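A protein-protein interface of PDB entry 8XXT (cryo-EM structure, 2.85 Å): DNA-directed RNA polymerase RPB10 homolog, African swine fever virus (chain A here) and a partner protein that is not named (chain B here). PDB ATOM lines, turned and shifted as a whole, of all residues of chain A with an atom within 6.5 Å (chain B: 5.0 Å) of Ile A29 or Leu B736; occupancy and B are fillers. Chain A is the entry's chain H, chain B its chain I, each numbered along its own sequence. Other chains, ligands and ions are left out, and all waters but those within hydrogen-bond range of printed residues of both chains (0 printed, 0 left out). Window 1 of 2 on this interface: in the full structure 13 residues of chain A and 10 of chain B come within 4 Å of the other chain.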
ATOM      1  N   ALA A  24      17.356  -9.164  24.774  1.00  0.00           N
ATOM      2  CA  ALA A  24      16.032  -9.660  24.420  1.00  0.00           C
ATOM      3  C   ALA A  24      15.124  -8.513  24.006  1.00  0.00           C
ATOM      4  O   ALA A  24      14.403  -8.608  23.008  1.00  0.00           O
ATOM      5  CB  ALA A  24      15.425 -10.435  25.585  1.00  0.00           C
ATOM      6  N   ARG A  25      15.170  -7.407  24.746  1.00  0.00           N
ATOM      7  CA  ARG A  25      14.388  -6.234  24.388  1.00  0.00           C
ATOM      8  C   ARG A  25      14.829  -5.673  23.047  1.00  0.00           C
ATOM      9  O   ARG A  25      13.991  -5.272  22.241  1.00  0.00           O
ATOM     10  CB  ARG A  25      14.507  -5.174  25.482  1.00  0.00           C
ATOM     11  CG  ARG A  25      13.908  -3.832  25.116  1.00  0.00           C
ATOM     12  CD  ARG A  25      14.050  -2.845  26.255  1.00  0.00           C
ATOM     13  NE  ARG A  25      15.445  -2.636  26.618  1.00  0.00           N
ATOM     14  CZ  ARG A  25      15.845  -1.983  27.699  1.00  0.00           C
ATOM     15  NH1 ARG A  25      14.979  -1.455  28.546  1.00  0.00           N
ATOM     16  NH2 ARG A  25      17.148  -1.858  27.936  1.00  0.00           N
ATOM     17  N   THR A  26      16.138  -5.634  22.790  1.00  0.00           N
ATOM     18  CA  THR A  26      16.618  -5.128  21.504  1.00  0.00           C
ATOM     19  C   THR A  26      16.075  -5.962  20.346  1.00  0.00           C
ATOM     20  O   THR A  26      15.548  -5.424  19.360  1.00  0.00           O
ATOM     21  CB  THR A  26      18.146  -5.118  21.486  1.00  0.00           C
ATOM     22  OG1 THR A  26      18.633  -4.295  22.550  1.00  0.00           O
ATOM     23  CG2 THR A  26      18.657  -4.575  20.169  1.00  0.00           C
ATOM     24  N   GLU A  27      16.181  -7.287  20.462  1.00  0.00           N
ATOM     25  CA  GLU A  27      15.641  -8.165  19.432  1.00  0.00           C
ATOM     26  C   GLU A  27      14.133  -8.013  19.309  1.00  0.00           C
ATOM     27  O   GLU A  27      13.581  -8.184  18.218  1.00  0.00           O
ATOM     28  CB  GLU A  27      16.009  -9.616  19.733  1.00  0.00           C
ATOM     29  CG  GLU A  27      17.505  -9.865  19.828  1.00  0.00           C
ATOM     30  CD  GLU A  27      17.836 -11.294  20.214  1.00  0.00           C
ATOM     31  OE1 GLU A  27      16.947 -12.163  20.103  1.00  0.00           O
ATOM     32  OE2 GLU A  27      18.986 -11.548  20.631  1.00  0.00           O
ATOM     33  N   TYR A  28      13.451  -7.691  20.408  1.00  0.00           N
ATOM     34  CA  TYR A  28      12.015  -7.455  20.338  1.00  0.00           C
ATOM     35  C   TYR A  28      11.692  -6.126  19.659  1.00  0.00           C
ATOM     36  O   TYR A  28      10.624  -5.985  19.057  1.00  0.00           O
ATOM     37  CB  TYR A  28      11.417  -7.518  21.742  1.00  0.00           C
ATOM     38  CG  TYR A  28       9.910  -7.524  21.785  1.00  0.00           C
ATOM     39  CD1 TYR A  28       9.195  -8.702  21.639  1.00  0.00           C
ATOM     40  CD2 TYR A  28       9.203  -6.358  22.002  1.00  0.00           C
ATOM     41  CE1 TYR A  28       7.814  -8.709  21.687  1.00  0.00           C
ATOM     42  CE2 TYR A  28       7.826  -6.353  22.052  1.00  0.00           C
ATOM     43  CZ  TYR A  28       7.137  -7.529  21.894  1.00  0.00           C
ATOM     44  OH  TYR A  28       5.764  -7.518  21.946  1.00  0.00           O
ATOM     45  N   ILE A  29      12.589  -5.138  19.758  1.00  0.00           N
ATOM     46  CA  ILE A  29      12.438  -3.917  18.965  1.00  0.00           C
ATOM     47  C   ILE A  29      12.551  -4.238  17.487  1.00  0.00           C
ATOM     48  O   ILE A  29      11.727  -3.807  16.674  1.00  0.00           O
ATOM     49  CB  ILE A  29      13.475  -2.844  19.352  1.00  0.00           C
ATOM     50  CG1 ILE A  29      13.696  -2.727  20.852  1.00  0.00           C
ATOM     51  CG2 ILE A  29      13.056  -1.492  18.792  1.00  0.00           C
ATOM     52  CD1 ILE A  29      12.442  -2.692  21.625  1.00  0.00           C
ATOM     53  N   LYS A  30      13.581  -5.002  17.119  1.00  0.00           N
ATOM     54  CA  LYS A  30      13.840  -5.230  15.703  1.00  0.00           C
ATOM     55  C   LYS A  30      12.676  -5.921  15.005  1.00  0.00           C
ATOM     56  O   LYS A  30      12.577  -5.853  13.776  1.00  0.00           O
ATOM     57  CB  LYS A  30      15.123  -6.039  15.526  1.00  0.00           C
ATOM     58  CG  LYS A  30      16.341  -5.398  16.168  1.00  0.00           C
ATOM     59  CD  LYS A  30      17.621  -5.798  15.462  1.00  0.00           C
ATOM     60  CE  LYS A  30      18.407  -6.808  16.277  1.00  0.00           C
ATOM     61  NZ  LYS A  30      17.786  -8.161  16.237  1.00  0.00           N
ATOM     62  N   THR A  31      11.789  -6.570  15.755  1.00  0.00           N
ATOM     63  CA  THR A  31      10.601  -7.193  15.188  1.00  0.00           C
ATOM     64  C   THR A  31       9.345  -6.346  15.352  1.00  0.00           C
ATOM     65  O   THR A  31       8.251  -6.830  15.046  1.00  0.00           O
ATOM     66  CB  THR A  31      10.363  -8.566  15.821  1.00  0.00           C
ATOM     67  OG1 THR A  31       9.796  -8.402  17.125  1.00  0.00           O
ATOM     68  CG2 THR A  31      11.664  -9.338  15.931  1.00  0.00           C
ATOM     69  N   LYS A  32       9.462  -5.109  15.828  1.00  0.00           N
ATOM     70  CA  LYS A  32       8.277  -4.280  16.021  1.00  0.00           C
ATOM     71  C   LYS A  32       8.446  -2.910  15.375  1.00  0.00           C
ATOM     72  O   LYS A  32       7.462  -2.293  14.954  1.00  0.00           O
ATOM     73  CB  LYS A  32       7.963  -4.142  17.513  1.00  0.00           C
ATOM     74  CG  LYS A  32       6.761  -3.262  17.832  1.00  0.00           C
ATOM     75  CD  LYS A  32       5.523  -3.695  17.060  1.00  0.00           C
ATOM     76  CE  LYS A  32       4.259  -3.554  17.894  1.00  0.00           C
ATOM     77  NZ  LYS A  32       3.936  -4.797  18.645  1.00  0.00           N
ATOM     78  N   MET A  33       9.680  -2.426  15.279  1.00  0.00           N
ATOM     79  CA  MET A  33       9.925  -1.112  14.697  1.00  0.00           C
ATOM     80  C   MET A  33       9.733  -1.127  13.185  1.00  0.00           C
ATOM     81  O   MET A  33       9.849  -2.165  12.534  1.00  0.00           O
ATOM     82  CB  MET A  33      11.334  -0.624  15.032  1.00  0.00           C
ATOM     83  CG  MET A  33      12.419  -1.229  14.168  1.00  0.00           C
ATOM     84  SD  MET A  33      14.065  -0.740  14.695  1.00  0.00           S
ATOM     85  CE  MET A  33      15.071  -1.860  13.731  1.00  0.00           C
ATOM     86  N   LEU A  47       8.618   3.907  22.285  1.00  0.00           N
ATOM     87  CA  LEU A  47       8.546   2.612  22.967  1.00  0.00           C
ATOM     88  C   LEU A  47       7.350   1.789  22.460  1.00  0.00           C
ATOM     89  O   LEU A  47       6.449   1.435  23.216  1.00  0.00           O
ATOM     90  CB  LEU A  47       8.532   2.834  24.482  1.00  0.00           C
ATOM     91  CG  LEU A  47       8.487   1.810  25.642  1.00  0.00           C
ATOM     92  CD1 LEU A  47       7.276   0.919  25.821  1.00  0.00           C
ATOM     93  CD2 LEU A  47       9.781   0.996  25.680  1.00  0.00           C
ATOM     94  N   ILE A  49       6.611  -0.968  22.151  1.00  0.00           N
ATOM     95  CA  ILE A  49       6.593  -2.346  22.592  1.00  0.00           C
ATOM     96  C   ILE A  49       5.712  -2.463  23.829  1.00  0.00           C
ATOM     97  O   ILE A  49       5.288  -1.470  24.424  1.00  0.00           O
ATOM     98  CB  ILE A  49       8.011  -2.826  22.925  1.00  0.00           C
ATOM     99  CG1 ILE A  49       8.760  -1.697  23.609  1.00  0.00           C
ATOM    100  CG2 ILE A  49       8.768  -3.075  21.647  1.00  0.00           C
ATOM    101  CD1 ILE A  49      10.164  -2.031  23.951  1.00  0.00           C
ATOM    102  N   LEU A  51       6.696  -4.951  27.129  1.00  0.00           N
ATOM    103  CA  LEU A  51       7.740  -5.863  27.572  1.00  0.00           C
ATOM    104  C   LEU A  51       7.284  -6.779  28.700  1.00  0.00           C
ATOM    105  O   LEU A  51       8.123  -7.407  29.351  1.00  0.00           O
ATOM    106  CB  LEU A  51       8.976  -5.077  28.003  1.00  0.00           C
ATOM    107  CG  LEU A  51       9.647  -4.252  26.907  1.00  0.00           C
ATOM    108  CD1 LEU A  51      10.467  -3.136  27.514  1.00  0.00           C
ATOM    109  CD2 LEU A  51      10.512  -5.125  26.027  1.00  0.00           C
ATOM    110  N   LYS A  78      24.885   2.887  25.729  1.00  0.00           N
ATOM    111  CA  LYS A  78      24.031   3.281  24.617  1.00  0.00           C
ATOM    112  C   LYS A  78      24.241   4.738  24.233  1.00  0.00           C
ATOM    113  O   LYS A  78      23.990   5.118  23.085  1.00  0.00           O
ATOM    114  CB  LYS A  78      22.562   3.045  24.970  1.00  0.00           C
ATOM    115  CG  LYS A  78      22.045   1.642  24.697  1.00  0.00           C
ATOM    116  CD  LYS A  78      22.725   0.604  25.568  1.00  0.00           C
ATOM    117  CE  LYS A  78      22.276  -0.795  25.208  1.00  0.00           C
ATOM    118  NZ  LYS A  78      20.805  -0.951  25.373  1.00  0.00           N
ATOM    119  N   GLU B 732      23.043   4.882  13.968  1.00  0.00           N
ATOM    120  CA  GLU B 732      21.684   4.359  14.069  1.00  0.00           C
ATOM    121  C   GLU B 732      21.663   3.039  14.829  1.00  0.00           C
ATOM    122  O   GLU B 732      20.713   2.756  15.568  1.00  0.00           O
ATOM    123  CB  GLU B 732      21.075   4.196  12.677  1.00  0.00           C
ATOM    124  CG  GLU B 732      19.569   4.442  12.609  1.00  0.00           C
ATOM    125  CD  GLU B 732      18.759   3.449  13.425  1.00  0.00           C
ATOM    126  OE1 GLU B 732      19.057   2.239  13.354  1.00  0.00           O
ATOM    127  OE2 GLU B 732      17.824   3.876  14.136  1.00  0.00           O
ATOM    128  N   GLN B 733      22.706   2.221  14.666  1.00  0.00           N
ATOM    129  CA  GLN B 733      22.779   0.968  15.408  1.00  0.00           C
ATOM    130  C   GLN B 733      22.766   1.224  16.909  1.00  0.00           C
ATOM    131  O   GLN B 733      22.043   0.555  17.657  1.00  0.00           O
ATOM    132  CB  GLN B 733      24.032   0.188  15.007  1.00  0.00           C
ATOM    133  CG  GLN B 733      24.550  -0.751  16.086  1.00  0.00           C
ATOM    134  CD  GLN B 733      25.863  -1.408  15.711  1.00  0.00           C
ATOM    135  OE1 GLN B 733      25.964  -2.088  14.690  1.00  0.00           O
ATOM    136  NE2 GLN B 733      26.876  -1.222  16.547  1.00  0.00           N
ATOM    137  N   LYS B 734      23.549   2.202  17.365  1.00  0.00           N
ATOM    138  CA  LYS B 734      23.500   2.588  18.771  1.00  0.00           C
ATOM    139  C   LYS B 734      22.147   3.185  19.130  1.00  0.00           C
ATOM    140  O   LYS B 734      21.632   2.951  20.229  1.00  0.00           O
ATOM    141  CB  LYS B 734      24.628   3.571  19.083  1.00  0.00           C
ATOM    142  CG  LYS B 734      26.021   2.990  18.911  1.00  0.00           C
ATOM    143  CD  LYS B 734      27.078   3.924  19.476  1.00  0.00           C
ATOM    144  CE  LYS B 734      26.938   4.068  20.982  1.00  0.00           C
ATOM    145  NZ  LYS B 734      27.277   2.806  21.691  1.00  0.00           N
ATOM    146  N   ALA B 735      21.559   3.966  18.218  1.00  0.00           N
ATOM    147  CA  ALA B 735      20.236   4.528  18.468  1.00  0.00           C
ATOM    148  C   ALA B 735      19.173   3.442  18.553  1.00  0.00           C
ATOM    149  O   ALA B 735      18.188   3.593  19.286  1.00  0.00           O
ATOM    150  CB  ALA B 735      19.877   5.539  17.380  1.00  0.00           C
ATOM    151  N   LEU B 736      19.341   2.354  17.800  1.00  0.00           N
ATOM    152  CA  LEU B 736      18.448   1.209  17.944  1.00  0.00           C
ATOM    153  C   LEU B 736      18.574   0.589  19.330  1.00  0.00           C
ATOM    154  O   LEU B 736      17.568   0.217  19.945  1.00  0.00           O
ATOM    155  CB  LEU B 736      18.744   0.177  16.857  1.00  0.00           C
ATOM    156  CG  LEU B 736      18.074  -1.193  16.972  1.00  0.00           C
ATOM    157  CD1 LEU B 736      16.571  -1.050  17.117  1.00  0.00           C
ATOM    158  CD2 LEU B 736      18.421  -2.053  15.768  1.00  0.00           C
ATOM    159  N   LEU B 737      19.801   0.477  19.842  1.00  0.00           N
ATOM    160  CA  LEU B 737      20.007  -0.062  21.180  1.00  0.00           C
ATOM    161  C   LEU B 737      19.439   0.849  22.262  1.00  0.00           C
ATOM    162  O   LEU B 737      19.303   0.419  23.411  1.00  0.00           O
ATOM    163  CB  LEU B 737      21.496  -0.296  21.424  1.00  0.00           C
ATOM    164  CG  LEU B 737      22.192  -1.249  20.454  1.00  0.00           C
ATOM    165  CD1 LEU B 737      23.685  -0.983  20.420  1.00  0.00           C
ATOM    166  CD2 LEU B 737      21.920  -2.689  20.831  1.00  0.00           C
ATOM    167  N   ALA B 738      19.108   2.096  21.921  1.00  0.00           N
ATOM    168  CA  ALA B 738      18.553   3.054  22.871  1.00  0.00           C
ATOM    169  C   ALA B 738      17.040   3.192  22.732  1.00  0.00           C
ATOM    170  O   ALA B 738      16.307   2.993  23.703  1.00  0.00           O
ATOM    171  CB  ALA B 738      19.232   4.418  22.695  1.00  0.00           C
ATOM    172  N   GLN B 739      16.558   3.536  21.539  1.00  0.00           N
ATOM    173  CA  GLN B 739      15.128   3.717  21.338  1.00  0.00           C
ATOM    174  C   GLN B 739      14.434   2.359  21.244  1.00  0.00           C
ATOM    175  O   GLN B 739      15.062   1.323  21.014  1.00  0.00           O
ATOM    176  CB  GLN B 739      14.866   4.550  20.087  1.00  0.00           C
ATOM    177  CG  GLN B 739      14.998   6.049  20.310  1.00  0.00           C
ATOM    178  CD  GLN B 739      13.722   6.682  20.837  1.00  0.00           C
ATOM    179  OE1 GLN B 739      13.132   6.211  21.807  1.00  0.00           O
ATOM    180  NE2 GLN B 739      13.288   7.756  20.191  1.00  0.00           N
ATOM    181  N   GLN B 740      13.110   2.367  21.438  1.00  0.00           N
ATOM    182  CA  GLN B 740      12.386   1.112  21.607  1.00  0.00           C
ATOM    183  C   GLN B 740      11.021   1.102  20.909  1.00  0.00           C
ATOM    184  O   GLN B 740      10.113   0.384  21.342  1.00  0.00           O
ATOM    185  CB  GLN B 740      12.208   0.801  23.097  1.00  0.00           C
ATOM    186  CG  GLN B 740      13.366   0.039  23.733  1.00  0.00           C
ATOM    187  CD  GLN B 740      14.221   0.895  24.648  1.00  0.00           C
ATOM    188  OE1 GLN B 740      13.745   1.418  25.653  1.00  0.00           O
ATOM    189  NE2 GLN B 740      15.500   1.014  24.316  1.00  0.00           N
ATOM    190  N   GLY B 741      10.855   1.862  19.828  1.00  0.00           N
ATOM    191  CA  GLY B 741       9.610   1.816  19.075  1.00  0.00           C
ATOM    192  C   GLY B 741       9.014   3.171  18.743  1.00  0.00           C
ATOM    193  O   GLY B 741       9.756   4.056  18.322  1.00  0.00           O
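The backbone carbonyl oxygen (O) of Leu B737 lies within hydrogen-bond range of the side-chain amino group (NZ) of Lys A78 (2.8 Å).
Arg A25 touches Gln B740 (CD to CG, 3.9 Å). Leu B737 touches Thr A26 (CD2 to CG2, 3.8 Å). Ile A29 touches Leu B736 (CG2 to CD1, 3.9 Å). CG of Gln B740 touches CD1 of Ile A29 (3.6 Å). Lys A30 touches Leu B736. Leu B736 touches Met A33. Leu A47 touches Gln B740. N of Leu A47 touches C of Gly B741, at 3.6 Å. CG1 of Ile A49 touches O of Gln B740, at 3.4 Å. Lys A78 touches Lys B734 (O to CE, 3.8 Å).
Thr A31 touches none of the printed residues of chain B. Of the printed residues of chain B, Met A33 touches Leu B736 (3.5 Å). Of the printed residues of chain B, Leu A47 touches Gln B740 (3.2 Å) and Gly B741 (3.6 Å). Of the printed residues of chain B, Ile A49 touches Gln B740. Glu B732 touches none of the printed residues of chain A. Printed residues of chain A within 4 Å of Lys B734: Lys A78. Of chain A, only Ile A29 (3.9 Å), Lys A30 (3.8 Å) and Met A33 (3.5 Å) come within 4 Å of Leu B736. The nearest residue of chain A that does not touch Leu B736 is Thr A26 (4.7 Å). The nearest printed residue of chain B that does not touch Lys A78 is Ala B738 (4.1 Å).
Of the 10 printed residues of chain B, 5 touch a printed residue of chain A. Of the 14 printed residues of chain A, 8 touch a printed residue of chain B. Printed residues of chain A that touch a printed residue of chain B: Arg A25, Thr A26, Ile A29, Lys A30, Met A33, Leu A47, Ile A49 and Lys A78. Hydrophobic or aromatic side chains of chain A that line the printed part of chain B: Ile A29, Met A33, Leu A47 and Ile A49. Along chain A the printed residues that touch a printed residue of chain B span positions 25 to 78.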
